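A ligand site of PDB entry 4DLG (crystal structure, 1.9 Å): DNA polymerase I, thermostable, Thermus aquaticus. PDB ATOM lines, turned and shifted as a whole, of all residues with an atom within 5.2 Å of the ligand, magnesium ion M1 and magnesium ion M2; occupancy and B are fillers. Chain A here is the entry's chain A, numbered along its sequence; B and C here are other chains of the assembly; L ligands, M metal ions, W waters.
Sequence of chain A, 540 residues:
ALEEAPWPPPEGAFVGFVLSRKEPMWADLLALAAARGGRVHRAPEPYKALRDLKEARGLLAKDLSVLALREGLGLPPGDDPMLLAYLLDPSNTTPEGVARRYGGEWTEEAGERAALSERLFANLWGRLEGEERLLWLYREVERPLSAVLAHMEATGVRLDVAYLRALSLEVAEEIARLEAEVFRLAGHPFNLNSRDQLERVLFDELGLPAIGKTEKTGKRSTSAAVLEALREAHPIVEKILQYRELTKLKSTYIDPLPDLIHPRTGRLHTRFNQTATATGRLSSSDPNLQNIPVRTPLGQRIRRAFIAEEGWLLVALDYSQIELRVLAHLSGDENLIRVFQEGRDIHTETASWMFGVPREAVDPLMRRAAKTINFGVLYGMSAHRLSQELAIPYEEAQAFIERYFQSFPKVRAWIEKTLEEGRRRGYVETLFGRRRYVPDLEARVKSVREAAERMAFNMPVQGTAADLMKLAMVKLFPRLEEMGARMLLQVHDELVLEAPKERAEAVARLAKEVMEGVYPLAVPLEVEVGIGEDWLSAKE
Magnesium ion M2 is bound by water W6 (2.1 Å), OD1 of Asp 493 (2.2 Å), OD2 of Asp 318 (2.2 Å) and O5 of the ligand (2.3 Å).
Water W6 bridges O4 of the ligand (3.0 Å) and OP2 of DOC 12 of chain C (3.5 Å).
Water W1 lies within hydrogen-bond range of the backbone carbonyl oxygen of Asp 318 and an oxygen (O10) of the ligand.
Water W4 bridges an oxygen (O4) of the ligand (2.8 Å) and OP1 of DOC 12 of chain C (3.1 Å).
Water W2 lies within hydrogen-bond range of the side-chain amino group (NZ) of Lys 371 (3.1 Å) and an oxygen (O12) of the ligand (3.2 Å).
Magnesium ion M1 is bound by an oxygen (O11) of the ligand (1.9 Å), the backbone carbonyl oxygen of Tyr 319 (1.9 Å), the side-chain carboxylate of Asp 318 (2.0 Å), an oxygen (O8) of the ligand (2.0 Å), the side-chain carboxylate of Asp 493 (2.1 Å) and an oxygen (O5) of the ligand (2.2 Å).
N4 of DOC 12 of chain C sits at hydrogen-bond distance from a nitrogen (N3) of the ligand.
N of Gln 321 lies within hydrogen-bond range of O10 of the ligand, 3.2 Å away.
An oxygen (O2) of the ligand lies within hydrogen-bond range of the guanidinium group of Arg 281 (3.1 Å).
NH1 of Arg 367 lies within salt-bridge range of O12 of the ligand, at 2.7 Å.
An oxygen (O12) of the ligand is in salt-bridge range of the side-chain amino group of Lys 371 (2.8 Å).
O6 of DG 4 of chain B is in hydrogen-bond range of a nitrogen (N3) of the ligand (3.2 Å).
An oxygen (O7) of the ligand lies within hydrogen-bond range of a ring nitrogen (NE2) of His 347 (2.9 Å).
Residues that only touch magnesium ion M2: DOC 12 of chain C (3.5 Å).
Three residues have an atom within 4 Å of magnesium ion M2: Asp 318, Asp 493 and DOC 12 of chain C.
The nearest printed residue that does not touch magnesium ion M2 is Glu 494 (4.5 Å).
Within 4 Å of magnesium ion M1: Asp 318, Tyr 319 and Asp 493.
N2 of DG 5 of chain B sits at hydrogen-bond distance from the guanidinium group of Arg 281 (3.4 Å).
The guanidinium group (NH1) of Arg 281 lies within hydrogen-bond range of O2 of DOC 12 of chain C, 2.7 Å away.
The side-chain carboxylate (OE2) of Glu 323 is in salt-bridge range of the guanidinium group (NH2) of Arg 281.
NZ of Lys 539 sits close to OD2 of Asp 318 (3.4 Å).
OE1 of Glu 323 is in hydrogen-bond range of OH of Tyr 379, 2.6 Å away.
O2 of DOC 12 of chain C lies close to N2 of DG 5 of chain B, 2.7 Å away.
O1 of the ligand lies close to N2 of DG 5 of chain B, at 3.3 Å.
CA of Ser 320 touches O10 of the ligand (3.4 Å).
Ile 322 touches the ligand.
Glu 323 touches the ligand.
CZ of Phe 375 touches O7 of the ligand, at 3.0 Å.
Of the 20 residues printed, 15 come within 4 Å of the ligand.
The nearest printed residue that does not touch the ligand is Thr 372 (4.1 Å).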
ATOM      1  N   ARG A 281      -9.955  26.290  -6.020  1.00  0.00           N
ATOM      2  CA  ARG A 281      -9.261  27.367  -5.339  1.00  0.00           C
ATOM      3  C   ARG A 281      -9.731  28.721  -5.865  1.00  0.00           C
ATOM      4  O   ARG A 281     -10.300  28.818  -6.949  1.00  0.00           O
ATOM      5  CB  ARG A 281      -7.750  27.263  -5.543  1.00  0.00           C
ATOM      6  CG  ARG A 281      -7.017  26.438  -4.487  1.00  0.00           C
ATOM      7  CD  ARG A 281      -5.512  26.648  -4.619  1.00  0.00           C
ATOM      8  NE  ARG A 281      -4.763  25.977  -3.565  1.00  0.00           N
ATOM      9  CZ  ARG A 281      -3.448  26.100  -3.395  1.00  0.00           C
ATOM     10  NH1 ARG A 281      -2.747  26.875  -4.206  1.00  0.00           N
ATOM     11  NH2 ARG A 281      -2.840  25.452  -2.407  1.00  0.00           N
ATOM     12  N   ASP A 318      -3.248  30.779   9.697  1.00  0.00           N
ATOM     13  CA  ASP A 318      -2.836  29.800   8.696  1.00  0.00           C
ATOM     14  C   ASP A 318      -3.112  28.378   9.170  1.00  0.00           C
ATOM     15  O   ASP A 318      -2.743  28.000  10.284  1.00  0.00           O
ATOM     16  CB  ASP A 318      -1.348  29.976   8.363  1.00  0.00           C
ATOM     17  CG  ASP A 318      -0.913  29.180   7.145  1.00  0.00           C
ATOM     18  OD1 ASP A 318      -1.395  28.052   6.955  1.00  0.00           O
ATOM     19  OD2 ASP A 318      -0.069  29.688   6.369  1.00  0.00           O
ATOM     20  N   TYR A 319      -3.751  27.592   8.312  1.00  0.00           N
ATOM     21  CA  TYR A 319      -3.967  26.165   8.583  1.00  0.00           C
ATOM     22  C   TYR A 319      -2.627  25.439   8.604  1.00  0.00           C
ATOM     23  O   TYR A 319      -1.771  25.664   7.750  1.00  0.00           O
ATOM     24  CB  TYR A 319      -4.866  25.540   7.528  1.00  0.00           C
ATOM     25  CG  TYR A 319      -6.348  25.723   7.754  1.00  0.00           C
ATOM     26  CD1 TYR A 319      -7.010  25.029   8.766  1.00  0.00           C
ATOM     27  CD2 TYR A 319      -7.095  26.585   6.966  1.00  0.00           C
ATOM     28  CE1 TYR A 319      -8.365  25.198   8.980  1.00  0.00           C
ATOM     29  CE2 TYR A 319      -8.452  26.758   7.163  1.00  0.00           C
ATOM     30  CZ  TYR A 319      -9.078  26.058   8.179  1.00  0.00           C
ATOM     31  OH  TYR A 319     -10.426  26.225   8.386  1.00  0.00           O
ATOM     32  N   SER A 320      -2.458  24.553   9.577  1.00  0.00           N
ATOM     33  CA  SER A 320      -1.218  23.781   9.719  1.00  0.00           C
ATOM     34  C   SER A 320      -1.297  22.439   9.010  1.00  0.00           C
ATOM     35  O   SER A 320      -2.125  21.600   9.345  1.00  0.00           O
ATOM     36  CB  SER A 320      -0.902  23.566  11.199  1.00  0.00           C
ATOM     37  OG  SER A 320      -0.163  22.371  11.394  1.00  0.00           O
ATOM     38  N   GLN A 321      -0.420  22.239   8.029  1.00  0.00           N
ATOM     39  CA  GLN A 321      -0.348  20.996   7.260  1.00  0.00           C
ATOM     40  C   GLN A 321      -1.698  20.585   6.685  1.00  0.00           C
ATOM     41  O   GLN A 321      -2.074  19.420   6.738  1.00  0.00           O
ATOM     42  CB  GLN A 321       0.246  19.872   8.111  1.00  0.00           C
ATOM     43  CG  GLN A 321       1.656  20.142   8.623  1.00  0.00           C
ATOM     44  CD  GLN A 321       1.742  20.103  10.136  1.00  0.00           C
ATOM     45  OE1 GLN A 321       1.590  21.123  10.813  1.00  0.00           O
ATOM     46  NE2 GLN A 321       1.993  18.920  10.681  1.00  0.00           N
ATOM     47  N   ILE A 322      -2.418  21.562   6.130  1.00  0.00           N
ATOM     48  CA  ILE A 322      -3.796  21.372   5.695  1.00  0.00           C
ATOM     49  C   ILE A 322      -4.001  20.222   4.700  1.00  0.00           C
ATOM     50  O   ILE A 322      -4.872  19.373   4.897  1.00  0.00           O
ATOM     51  CB  ILE A 322      -4.417  22.692   5.152  1.00  0.00           C
ATOM     52  CG1 ILE A 322      -5.842  22.455   4.643  1.00  0.00           C
ATOM     53  CG2 ILE A 322      -3.539  23.319   4.083  1.00  0.00           C
ATOM     54  CD1 ILE A 322      -6.818  22.030   5.722  1.00  0.00           C
ATOM     55  N   GLU A 323      -3.183  20.171   3.646  1.00  0.00           N
ATOM     56  CA  GLU A 323      -3.352  19.124   2.630  1.00  0.00           C
ATOM     57  C   GLU A 323      -2.877  17.757   3.099  1.00  0.00           C
ATOM     58  O   GLU A 323      -3.330  16.721   2.583  1.00  0.00           O
ATOM     59  CB  GLU A 323      -2.656  19.521   1.325  1.00  0.00           C
ATOM     60  CG  GLU A 323      -3.370  20.630   0.569  1.00  0.00           C
ATOM     61  CD  GLU A 323      -2.872  20.791  -0.852  1.00  0.00           C
ATOM     62  OE1 GLU A 323      -2.012  19.987  -1.279  1.00  0.00           O
ATOM     63  OE2 GLU A 323      -3.325  21.728  -1.539  1.00  0.00           O
ATOM     64  N   HIS A 347       6.599  18.528   8.272  1.00  0.00           N
ATOM     65  CA  HIS A 347       7.441  19.570   7.719  1.00  0.00           C
ATOM     66  C   HIS A 347       8.709  19.782   8.537  1.00  0.00           C
ATOM     67  O   HIS A 347       9.781  20.045   8.000  1.00  0.00           O
ATOM     68  CB  HIS A 347       6.670  20.888   7.614  1.00  0.00           C
ATOM     69  CG  HIS A 347       5.557  20.862   6.605  1.00  0.00           C
ATOM     70  ND1 HIS A 347       5.429  19.866   5.670  1.00  0.00           N
ATOM     71  CD2 HIS A 347       4.514  21.707   6.407  1.00  0.00           C
ATOM     72  CE1 HIS A 347       4.372  20.099   4.919  1.00  0.00           C
ATOM     73  NE2 HIS A 347       3.796  21.207   5.347  1.00  0.00           N
ATOM     74  N   ARG A 367      12.210  24.951   7.726  1.00  0.00           N
ATOM     75  CA  ARG A 367      10.933  24.251   7.707  1.00  0.00           C
ATOM     76  C   ARG A 367      10.165  24.485   6.405  1.00  0.00           C
ATOM     77  O   ARG A 367       9.574  23.564   5.857  1.00  0.00           O
ATOM     78  CB  ARG A 367      10.078  24.659   8.911  1.00  0.00           C
ATOM     79  CG  ARG A 367       8.757  23.906   9.009  1.00  0.00           C
ATOM     80  CD  ARG A 367       7.921  24.407  10.169  1.00  0.00           C
ATOM     81  NE  ARG A 367       6.649  23.691  10.266  1.00  0.00           N
ATOM     82  CZ  ARG A 367       5.546  24.038   9.612  1.00  0.00           C
ATOM     83  NH1 ARG A 367       5.557  25.091   8.804  1.00  0.00           N
ATOM     84  NH2 ARG A 367       4.440  23.329   9.759  1.00  0.00           N
ATOM     85  N   LYS A 371       8.665  22.056   2.782  1.00  0.00           N
ATOM     86  CA  LYS A 371       7.315  22.009   2.240  1.00  0.00           C
ATOM     87  C   LYS A 371       7.318  21.566   0.780  1.00  0.00           C
ATOM     88  O   LYS A 371       6.511  20.737   0.373  1.00  0.00           O
ATOM     89  CB  LYS A 371       6.629  23.377   2.358  1.00  0.00           C
ATOM     90  CG  LYS A 371       6.404  23.836   3.781  1.00  0.00           C
ATOM     91  CD  LYS A 371       5.634  25.147   3.812  1.00  0.00           C
ATOM     92  CE  LYS A 371       5.364  25.607   5.225  1.00  0.00           C
ATOM     93  NZ  LYS A 371       4.553  26.860   5.257  1.00  0.00           N
ATOM     94  N   THR A 372       8.247  22.116   0.004  1.00  0.00           N
ATOM     95  CA  THR A 372       8.400  21.770  -1.396  1.00  0.00           C
ATOM     96  C   THR A 372       8.742  20.290  -1.537  1.00  0.00           C
ATOM     97  O   THR A 372       8.386  19.633  -2.519  1.00  0.00           O
ATOM     98  CB  THR A 372       9.501  22.612  -2.071  1.00  0.00           C
ATOM     99  OG1 THR A 372       9.232  24.001  -1.853  1.00  0.00           O
ATOM    100  CG2 THR A 372       9.555  22.340  -3.576  1.00  0.00           C
ATOM    101  N   PHE A 375       5.387  18.059  -0.161  1.00  0.00           N
ATOM    102  CA  PHE A 375       4.311  18.172  -1.137  1.00  0.00           C
ATOM    103  C   PHE A 375       4.774  17.694  -2.509  1.00  0.00           C
ATOM    104  O   PHE A 375       3.998  17.096  -3.251  1.00  0.00           O
ATOM    105  CB  PHE A 375       3.812  19.617  -1.215  1.00  0.00           C
ATOM    106  CG  PHE A 375       3.233  20.121   0.070  1.00  0.00           C
ATOM    107  CD1 PHE A 375       2.453  19.288   0.864  1.00  0.00           C
ATOM    108  CD2 PHE A 375       3.454  21.422   0.495  1.00  0.00           C
ATOM    109  CE1 PHE A 375       1.909  19.742   2.049  1.00  0.00           C
ATOM    110  CE2 PHE A 375       2.924  21.876   1.678  1.00  0.00           C
ATOM    111  CZ  PHE A 375       2.142  21.037   2.459  1.00  0.00           C
ATOM    112  N   TYR A 379       3.073  14.361  -4.627  1.00  0.00           N
ATOM    113  CA  TYR A 379       2.377  14.445  -5.912  1.00  0.00           C
ATOM    114  C   TYR A 379       3.257  14.038  -7.097  1.00  0.00           C
ATOM    115  O   TYR A 379       3.195  14.653  -8.168  1.00  0.00           O
ATOM    116  CB  TYR A 379       1.800  15.845  -6.130  1.00  0.00           C
ATOM    117  CG  TYR A 379       0.856  16.274  -5.031  1.00  0.00           C
ATOM    118  CD1 TYR A 379      -0.350  15.615  -4.821  1.00  0.00           C
ATOM    119  CD2 TYR A 379       1.156  17.348  -4.211  1.00  0.00           C
ATOM    120  CE1 TYR A 379      -1.223  15.998  -3.821  1.00  0.00           C
ATOM    121  CE2 TYR A 379       0.297  17.756  -3.209  1.00  0.00           C
ATOM    122  CZ  TYR A 379      -0.890  17.079  -3.017  1.00  0.00           C
ATOM    123  OH  TYR A 379      -1.750  17.472  -2.024  1.00  0.00           O
ATOM    124  N   VAL A 491      -5.379  33.675   1.297  1.00  0.00           N
ATOM    125  CA  VAL A 491      -4.259  33.088   0.578  1.00  0.00           C
ATOM    126  C   VAL A 491      -4.317  31.560   0.652  1.00  0.00           C
ATOM    127  O   VAL A 491      -3.491  30.928   1.318  1.00  0.00           O
ATOM    128  CB  VAL A 491      -2.898  33.588   1.104  1.00  0.00           C
ATOM    129  CG1 VAL A 491      -1.803  33.318   0.083  1.00  0.00           C
ATOM    130  CG2 VAL A 491      -2.976  35.080   1.411  1.00  0.00           C
ATOM    131  N   ASP A 493      -4.823  28.847   2.120  1.00  0.00           N
ATOM    132  CA  ASP A 493      -5.056  28.297   3.463  1.00  0.00           C
ATOM    133  C   ASP A 493      -4.814  29.353   4.534  1.00  0.00           C
ATOM    134  O   ASP A 493      -4.623  29.037   5.710  1.00  0.00           O
ATOM    135  CB  ASP A 493      -4.200  27.047   3.706  1.00  0.00           C
ATOM    136  CG  ASP A 493      -2.758  27.370   4.079  1.00  0.00           C
ATOM    137  OD1 ASP A 493      -2.215  28.401   3.623  1.00  0.00           O
ATOM    138  OD2 ASP A 493      -2.157  26.557   4.814  1.00  0.00           O
ATOM    139  N   GLU A 494      -4.837  30.620   4.129  1.00  0.00           N
ATOM    140  CA  GLU A 494      -4.544  31.721   5.039  1.00  0.00           C
ATOM    141  C   GLU A 494      -5.592  32.834   4.957  1.00  0.00           C
ATOM    142  O   GLU A 494      -6.096  33.147   3.877  1.00  0.00           O
ATOM    143  CB  GLU A 494      -3.150  32.297   4.744  1.00  0.00           C
ATOM    144  CG  GLU A 494      -2.734  33.426   5.662  1.00  0.00           C
ATOM    145  CD  GLU A 494      -1.396  34.018   5.290  1.00  0.00           C
ATOM    146  OE1 GLU A 494      -0.691  33.421   4.443  1.00  0.00           O
ATOM    147  OE2 GLU A 494      -1.039  35.081   5.841  1.00  0.00           O
ATOM    148  N   LYS A 539       2.731  37.213  11.295  1.00  0.00           N
ATOM    149  CA  LYS A 539       3.000  35.782  11.159  1.00  0.00           C
ATOM    150  C   LYS A 539       4.310  35.410  11.855  1.00  0.00           C
ATOM    151  O   LYS A 539       5.090  34.612  11.336  1.00  0.00           O
ATOM    152  CB  LYS A 539       3.044  35.374   9.693  1.00  0.00           C
ATOM    153  CG  LYS A 539       1.759  35.674   8.923  1.00  0.00           C
ATOM    154  CD  LYS A 539       1.699  34.898   7.621  1.00  0.00           C
ATOM    155  CE  LYS A 539       1.647  33.405   7.874  1.00  0.00           C
ATOM    156  NZ  LYS A 539       1.579  32.622   6.608  1.00  0.00           N
ATOM    157  P    DG B   4       9.085  16.310 -11.591  1.00  0.00           P
ATOM    158  OP1  DG B   4      10.544  16.364 -11.389  1.00  0.00           O
ATOM    159  OP2  DG B   4       8.411  15.000 -11.725  1.00  0.00           O
ATOM    160  O5'  DG B   4       8.369  17.081 -10.390  1.00  0.00           O
ATOM    161  C5'  DG B   4       7.176  17.830 -10.646  1.00  0.00           C
ATOM    162  C4'  DG B   4       5.966  17.214  -9.979  1.00  0.00           C
ATOM    163  O4'  DG B   4       6.241  17.021  -8.566  1.00  0.00           O
ATOM    164  C3'  DG B   4       4.705  18.065 -10.060  1.00  0.00           C
ATOM    165  O3'  DG B   4       3.910  17.612 -11.145  1.00  0.00           O
ATOM    166  C2'  DG B   4       4.017  17.792  -8.724  1.00  0.00           C
ATOM    167  C1'  DG B   4       5.205  17.578  -7.783  1.00  0.00           C
ATOM    168  N9   DG B   4       5.710  18.802  -7.171  1.00  0.00           N
ATOM    169  C8   DG B   4       6.944  19.368  -7.351  1.00  0.00           C
ATOM    170  N7   DG B   4       7.121  20.470  -6.666  1.00  0.00           N
ATOM    171  C5   DG B   4       5.915  20.635  -5.988  1.00  0.00           C
ATOM    172  C6   DG B   4       5.520  21.657  -5.095  1.00  0.00           C
ATOM    173  O6   DG B   4       6.168  22.636  -4.707  1.00  0.00           O
ATOM    174  N1   DG B   4       4.219  21.458  -4.631  1.00  0.00           N
ATOM    175  C2   DG B   4       3.406  20.399  -4.989  1.00  0.00           C
ATOM    176  N2   DG B   4       2.185  20.375  -4.443  1.00  0.00           N
ATOM    177  N3   DG B   4       3.772  19.438  -5.835  1.00  0.00           N
ATOM    178  C4   DG B   4       5.033  19.617  -6.284  1.00  0.00           C
ATOM    179  P    DG B   5       3.242  18.673 -12.151  1.00  0.00           P
ATOM    180  OP1  DG B   5       2.795  17.944 -13.353  1.00  0.00           O
ATOM    181  OP2  DG B   5       4.171  19.817 -12.286  1.00  0.00           O
ATOM    182  O5'  DG B   5       1.957  19.198 -11.357  1.00  0.00           O
ATOM    183  C5'  DG B   5       0.862  18.314 -11.086  1.00  0.00           C
ATOM    184  C4'  DG B   5      -0.106  18.924 -10.096  1.00  0.00           C
ATOM    185  O4'  DG B   5       0.564  19.126  -8.825  1.00  0.00           O
ATOM    186  C3'  DG B   5      -0.645  20.302 -10.474  1.00  0.00           C
ATOM    187  O3'  DG B   5      -1.806  20.160 -11.283  1.00  0.00           O
ATOM    188  C2'  DG B   5      -1.000  20.892  -9.120  1.00  0.00           C
ATOM    189  C1'  DG B   5       0.088  20.305  -8.209  1.00  0.00           C
ATOM    190  N9   DG B   5       1.199  21.217  -7.986  1.00  0.00           N
ATOM    191  C8   DG B   5       2.461  21.151  -8.521  1.00  0.00           C
ATOM    192  N7   DG B   5       3.244  22.119  -8.141  1.00  0.00           N
ATOM    193  C5   DG B   5       2.457  22.877  -7.283  1.00  0.00           C
ATOM    194  C6   DG B   5       2.753  24.053  -6.555  1.00  0.00           C
ATOM    195  O6   DG B   5       3.821  24.674  -6.516  1.00  0.00           O
ATOM    196  N1   DG B   5       1.671  24.492  -5.807  1.00  0.00           N
ATOM    197  C2   DG B   5       0.436  23.876  -5.768  1.00  0.00           C
ATOM    198  N2   DG B   5      -0.496  24.449  -5.000  1.00  0.00           N
ATOM    199  N3   DG B   5       0.139  22.777  -6.444  1.00  0.00           N
ATOM    200  C4   DG B   5       1.188  22.331  -7.176  1.00  0.00           C
ATOM    201  N1  DOC C  12       1.274  28.051  -2.326  1.00  0.00           N
ATOM    202  C2  DOC C  12       1.067  27.072  -3.304  1.00  0.00           C
ATOM    203  N3  DOC C  12       2.114  26.582  -4.008  1.00  0.00           N
ATOM    204  C4  DOC C  12       3.366  27.027  -3.762  1.00  0.00           C
ATOM    205  C5  DOC C  12       3.586  27.992  -2.796  1.00  0.00           C
ATOM    206  C6  DOC C  12       2.507  28.489  -2.066  1.00  0.00           C
ATOM    207  O2  DOC C  12      -0.091  26.653  -3.537  1.00  0.00           O
ATOM    208  N4  DOC C  12       4.405  26.535  -4.472  1.00  0.00           N
ATOM    209  C1' DOC C  12       0.143  28.581  -1.557  1.00  0.00           C
ATOM    210  C2' DOC C  12       0.006  27.809  -0.245  1.00  0.00           C
ATOM    211  C3' DOC C  12       0.161  28.837   0.859  1.00  0.00           C
ATOM    212  C4' DOC C  12       0.100  30.180   0.159  1.00  0.00           C
ATOM    213  O4' DOC C  12       0.389  29.943  -1.224  1.00  0.00           O
ATOM    214  C5' DOC C  12       1.121  31.136   0.759  1.00  0.00           C
ATOM    215  O5' DOC C  12       2.427  30.596   0.609  1.00  0.00           O
ATOM    216  P   DOC C  12       3.716  31.474   1.039  1.00  0.00           P
ATOM    217  OP1 DOC C  12       4.956  30.631   0.862  1.00  0.00           O
ATOM    218  OP2 DOC C  12       3.407  32.105   2.375  1.00  0.00           O
HETATM  219  N1  LIG L   1       1.231  23.744  -1.115  1.00  0.00           N
HETATM  220  C1  LIG L   1       1.730  23.079  -2.222  1.00  0.00           C
HETATM  221  N2  LIG L   1       3.050  23.239  -2.577  1.00  0.00           N
HETATM  222  C2  LIG L   1       3.877  24.061  -1.834  1.00  0.00           C
HETATM  223  C3  LIG L   1       3.365  24.717  -0.721  1.00  0.00           C
HETATM  224  C4  LIG L   1       2.037  24.554  -0.370  1.00  0.00           C
HETATM  225  O1  LIG L   1       1.000  22.356  -2.883  1.00  0.00           O
HETATM  226  N3  LIG L   1       5.150  24.213  -2.171  1.00  0.00           N
HETATM  227  C5  LIG L   1      -0.185  23.572  -0.739  1.00  0.00           C
HETATM  228  C6  LIG L   1      -0.284  22.582   0.414  1.00  0.00           C
HETATM  229  C7  LIG L   1      -0.961  23.328   1.550  1.00  0.00           C
HETATM  230  C8  LIG L   1      -1.345  24.680   0.972  1.00  0.00           C
HETATM  231  O2  LIG L   1      -0.717  24.808  -0.281  1.00  0.00           O
HETATM  232  C9  LIG L   1      -0.917  25.790   1.921  1.00  0.00           C
HETATM  233  O3  LIG L   1       0.488  25.902   1.941  1.00  0.00           O
HETATM  234  P1  LIG L   1       1.291  26.090   3.324  1.00  0.00           P
HETATM  235  O4  LIG L   1       2.535  26.902   3.079  1.00  0.00           O
HETATM  236  O5  LIG L   1       0.435  26.734   4.392  1.00  0.00           O
HETATM  237  O6  LIG L   1       1.697  24.595   3.743  1.00  0.00           O
HETATM  238  P2  LIG L   1       1.248  23.950   5.146  1.00  0.00           P
HETATM  239  O7  LIG L   1       1.223  22.451   4.999  1.00  0.00           O
HETATM  240  O8  LIG L   1      -0.095  24.472   5.591  1.00  0.00           O
HETATM  241  O9  LIG L   1       2.413  24.370   6.167  1.00  0.00           O
HETATM  242  P3  LIG L   1       2.144  25.293   7.460  1.00  0.00           P
HETATM  243  O10 LIG L   1       1.926  24.392   8.646  1.00  0.00           O
HETATM  244  O11 LIG L   1       0.924  26.152   7.236  1.00  0.00           O
HETATM  245  O12 LIG L   1       3.342  26.167   7.726  1.00  0.00           O
HETATM  246 MG    MG M   1      -0.712  26.305   6.264  1.00  0.00          MG
HETATM  247 MG    MG M   2      -0.258  28.906   4.370  1.00  0.00          MG
HETATM  248  O   HOH W   1       0.384  27.172   9.684  1.00  0.00           O
HETATM  249  O   HOH W   2       2.616  28.950   6.365  1.00  0.00           O
HETATM  250  O   HOH W   3      -1.765  21.271  -3.992  1.00  0.00           O
HETATM  251  O   HOH W   4       4.620  27.638   1.436  1.00  0.00           O
HETATM  252  O   HOH W   5       6.386  26.077  -0.735  1.00  0.00           O
HETATM  253  O   HOH W   6       1.667  29.611   4.016  1.00  0.00           O
